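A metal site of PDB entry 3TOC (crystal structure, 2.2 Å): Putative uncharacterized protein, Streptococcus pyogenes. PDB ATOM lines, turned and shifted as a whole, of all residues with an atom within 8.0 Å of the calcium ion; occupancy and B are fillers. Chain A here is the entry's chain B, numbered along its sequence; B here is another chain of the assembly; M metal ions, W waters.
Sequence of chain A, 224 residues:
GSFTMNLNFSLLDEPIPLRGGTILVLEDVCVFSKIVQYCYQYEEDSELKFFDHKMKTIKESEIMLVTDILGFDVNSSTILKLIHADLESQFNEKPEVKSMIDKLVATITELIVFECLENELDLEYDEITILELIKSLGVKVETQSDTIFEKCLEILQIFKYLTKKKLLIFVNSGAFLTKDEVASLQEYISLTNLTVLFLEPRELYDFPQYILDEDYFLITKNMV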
ATOM      1  N   TYR A 125     -19.190 -30.509  16.219  1.00  0.00           N
ATOM      2  CA  TYR A 125     -19.700 -29.232  16.710  1.00  0.00           C
ATOM      3  C   TYR A 125     -18.942 -28.856  17.976  1.00  0.00           C
ATOM      4  O   TYR A 125     -18.214 -29.690  18.535  1.00  0.00           O
ATOM      5  CB  TYR A 125     -21.177 -29.380  17.048  1.00  0.00           C
ATOM      6  CG  TYR A 125     -21.436 -30.625  17.855  1.00  0.00           C
ATOM      7  CD1 TYR A 125     -21.755 -31.829  17.223  1.00  0.00           C
ATOM      8  CD2 TYR A 125     -21.322 -30.624  19.241  1.00  0.00           C
ATOM      9  CE1 TYR A 125     -21.975 -32.984  17.944  1.00  0.00           C
ATOM     10  CE2 TYR A 125     -21.547 -31.773  19.968  1.00  0.00           C
ATOM     11  CZ  TYR A 125     -21.858 -32.958  19.305  1.00  0.00           C
ATOM     12  OH  TYR A 125     -22.075 -34.115  19.997  1.00  0.00           O
ATOM     13  N   ASP A 126     -19.095 -27.614  18.435  1.00  0.00           N
ATOM     14  CA  ASP A 126     -18.476 -27.215  19.704  1.00  0.00           C
ATOM     15  C   ASP A 126     -19.524 -26.985  20.795  1.00  0.00           C
ATOM     16  O   ASP A 126     -19.955 -27.938  21.423  1.00  0.00           O
ATOM     17  CB  ASP A 126     -17.511 -26.032  19.557  1.00  0.00           C
ATOM     18  CG  ASP A 126     -18.017 -24.980  18.618  1.00  0.00           C
ATOM     19  OD1 ASP A 126     -17.674 -25.028  17.417  1.00  0.00           O
ATOM     20  OD2 ASP A 126     -18.738 -24.081  19.070  1.00  0.00           O
ATOM     21  N   GLU A 127     -19.940 -25.750  21.027  1.00  0.00           N
ATOM     22  CA  GLU A 127     -20.908 -25.533  22.100  1.00  0.00           C
ATOM     23  C   GLU A 127     -21.552 -24.205  21.918  1.00  0.00           C
ATOM     24  O   GLU A 127     -20.967 -23.336  21.317  1.00  0.00           O
ATOM     25  CB  GLU A 127     -20.185 -25.509  23.432  1.00  0.00           C
ATOM     26  CG  GLU A 127     -19.218 -24.358  23.503  1.00  0.00           C
ATOM     27  CD  GLU A 127     -18.535 -24.263  24.842  1.00  0.00           C
ATOM     28  OE1 GLU A 127     -18.829 -25.111  25.715  1.00  0.00           O
ATOM     29  OE2 GLU A 127     -17.714 -23.335  25.029  1.00  0.00           O
ATOM     30  N   ILE A 128     -22.751 -24.027  22.454  1.00  0.00           N
ATOM     31  CA  ILE A 128     -23.393 -22.722  22.426  1.00  0.00           C
ATOM     32  C   ILE A 128     -23.062 -21.973  23.718  1.00  0.00           C
ATOM     33  O   ILE A 128     -23.216 -22.518  24.811  1.00  0.00           O
ATOM     34  CB  ILE A 128     -24.901 -22.889  22.271  1.00  0.00           C
ATOM     35  CG1 ILE A 128     -25.188 -23.614  20.958  1.00  0.00           C
ATOM     36  CG2 ILE A 128     -25.607 -21.549  22.303  1.00  0.00           C
ATOM     37  CD1 ILE A 128     -26.672 -23.930  20.745  1.00  0.00           C
ATOM     38  N   THR A 129     -22.564 -20.740  23.606  1.00  0.00           N
ATOM     39  CA  THR A 129     -22.179 -19.975  24.788  1.00  0.00           C
ATOM     40  C   THR A 129     -23.215 -18.878  25.091  1.00  0.00           C
ATOM     41  O   THR A 129     -24.037 -18.549  24.229  1.00  0.00           O
ATOM     42  CB  THR A 129     -20.792 -19.358  24.615  1.00  0.00           C
ATOM     43  OG1 THR A 129     -20.883 -18.230  23.717  1.00  0.00           O
ATOM     44  CG2 THR A 129     -19.814 -20.401  24.052  1.00  0.00           C
ATOM     45  N   GLU A 132     -22.878 -15.977  22.796  1.00  0.00           N
ATOM     46  CA  GLU A 132     -23.505 -16.301  21.505  1.00  0.00           C
ATOM     47  C   GLU A 132     -25.019 -16.152  21.485  1.00  0.00           C
ATOM     48  O   GLU A 132     -25.587 -15.713  20.489  1.00  0.00           O
ATOM     49  CB  GLU A 132     -23.106 -17.713  21.062  1.00  0.00           C
ATOM     50  CG  GLU A 132     -21.645 -17.801  20.674  1.00  0.00           C
ATOM     51  CD  GLU A 132     -21.213 -19.209  20.349  1.00  0.00           C
ATOM     52  OE1 GLU A 132     -21.773 -20.157  20.956  1.00  0.00           O
ATOM     53  OE2 GLU A 132     -20.332 -19.362  19.479  1.00  0.00           O
ATOM     54  N   LEU B 133     -28.905 -20.765  16.475  1.00  0.00           N
ATOM     55  CA  LEU B 133     -28.423 -21.760  17.416  1.00  0.00           C
ATOM     56  C   LEU B 133     -27.508 -22.754  16.717  1.00  0.00           C
ATOM     57  O   LEU B 133     -26.445 -23.097  17.212  1.00  0.00           O
ATOM     58  CB  LEU B 133     -29.602 -22.490  18.044  1.00  0.00           C
ATOM     59  CG  LEU B 133     -30.443 -21.559  18.922  1.00  0.00           C
ATOM     60  CD1 LEU B 133     -31.609 -22.320  19.560  1.00  0.00           C
ATOM     61  CD2 LEU B 133     -29.603 -20.893  20.005  1.00  0.00           C
ATOM     62  N   ILE B 134     -27.937 -23.223  15.566  1.00  0.00           N
ATOM     63  CA  ILE B 134     -27.161 -24.170  14.807  1.00  0.00           C
ATOM     64  C   ILE B 134     -25.813 -23.573  14.386  1.00  0.00           C
ATOM     65  O   ILE B 134     -24.763 -24.213  14.527  1.00  0.00           O
ATOM     66  CB  ILE B 134     -27.954 -24.677  13.603  1.00  0.00           C
ATOM     67  CG1 ILE B 134     -29.068 -25.603  14.105  1.00  0.00           C
ATOM     68  CG2 ILE B 134     -27.028 -25.417  12.643  1.00  0.00           C
ATOM     69  CD1 ILE B 134     -30.092 -25.942  13.045  1.00  0.00           C
ATOM     70  N   LYS B 135     -25.830 -22.347  13.878  1.00  0.00           N
ATOM     71  CA  LYS B 135     -24.568 -21.689  13.539  1.00  0.00           C
ATOM     72  C   LYS B 135     -23.684 -21.547  14.780  1.00  0.00           C
ATOM     73  O   LYS B 135     -22.483 -21.803  14.733  1.00  0.00           O
ATOM     74  CB  LYS B 135     -24.804 -20.321  12.909  1.00  0.00           C
ATOM     75  CG  LYS B 135     -25.544 -20.354  11.589  1.00  0.00           C
ATOM     76  CD  LYS B 135     -25.574 -18.949  10.989  1.00  0.00           C
ATOM     77  CE  LYS B 135     -26.762 -18.733  10.051  1.00  0.00           C
ATOM     78  NZ  LYS B 135     -26.490 -19.157   8.639  1.00  0.00           N
ATOM     79  N   SER B 136     -24.278 -21.147  15.894  1.00  0.00           N
ATOM     80  CA  SER B 136     -23.493 -20.894  17.077  1.00  0.00           C
ATOM     81  C   SER B 136     -22.865 -22.153  17.614  1.00  0.00           C
ATOM     82  O   SER B 136     -21.830 -22.103  18.261  1.00  0.00           O
ATOM     83  CB  SER B 136     -24.366 -20.283  18.184  1.00  0.00           C
ATOM     84  OG  SER B 136     -24.894 -19.046  17.784  1.00  0.00           O
ATOM     85  N   LEU B 137     -23.521 -23.276  17.376  1.00  0.00           N
ATOM     86  CA  LEU B 137     -23.040 -24.552  17.902  1.00  0.00           C
ATOM     87  C   LEU B 137     -21.790 -25.032  17.130  1.00  0.00           C
ATOM     88  O   LEU B 137     -21.028 -25.870  17.619  1.00  0.00           O
ATOM     89  CB  LEU B 137     -24.152 -25.596  17.893  1.00  0.00           C
ATOM     90  CG  LEU B 137     -23.805 -27.016  18.327  1.00  0.00           C
ATOM     91  CD1 LEU B 137     -23.181 -27.027  19.713  1.00  0.00           C
ATOM     92  CD2 LEU B 137     -25.059 -27.867  18.284  1.00  0.00           C
ATOM     93  N   GLY B 138     -21.580 -24.474  15.952  1.00  0.00           N
ATOM     94  CA  GLY B 138     -20.359 -24.704  15.191  1.00  0.00           C
ATOM     95  C   GLY B 138     -20.369 -26.010  14.451  1.00  0.00           C
ATOM     96  O   GLY B 138     -19.341 -26.662  14.331  1.00  0.00           O
ATOM     97  N   VAL B 139     -21.541 -26.395  13.949  1.00  0.00           N
ATOM     98  CA  VAL B 139     -21.726 -27.665  13.270  1.00  0.00           C
ATOM     99  C   VAL B 139     -21.019 -27.688  11.922  1.00  0.00           C
ATOM    100  O   VAL B 139     -21.171 -26.789  11.120  1.00  0.00           O
ATOM    101  CB  VAL B 139     -23.207 -28.021  13.089  1.00  0.00           C
ATOM    102  CG1 VAL B 139     -23.344 -29.317  12.287  1.00  0.00           C
ATOM    103  CG2 VAL B 139     -23.860 -28.187  14.454  1.00  0.00           C
HETATM  104 CA    CA M   1     -19.917 -21.829  19.743  1.00  0.00          CA
HETATM  105  O   HOH W   1     -17.729 -21.848  21.593  1.00  0.00           O
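The calcium ion is bound by O of Glu 127, O of Ser 136 of chain B, OE2 of Glu 132, OD2 of Asp 126, OE1 of Glu 132 and water W1.
Of the 13 residues printed, 4 come within 4 Å of the calcium ion.
The nearest printed residue that does not touch the calcium ion is Ile 128 (4.5 Å).
The backbone NH of Glu 132 is in hydrogen-bond range of the side-chain hydroxyl of Thr 129 (3.1 Å).
The backbone carbonyl oxygen of Leu 137 of chain B lies within hydrogen-bond range of the backbone NH of Asp 126 (2.7 Å).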
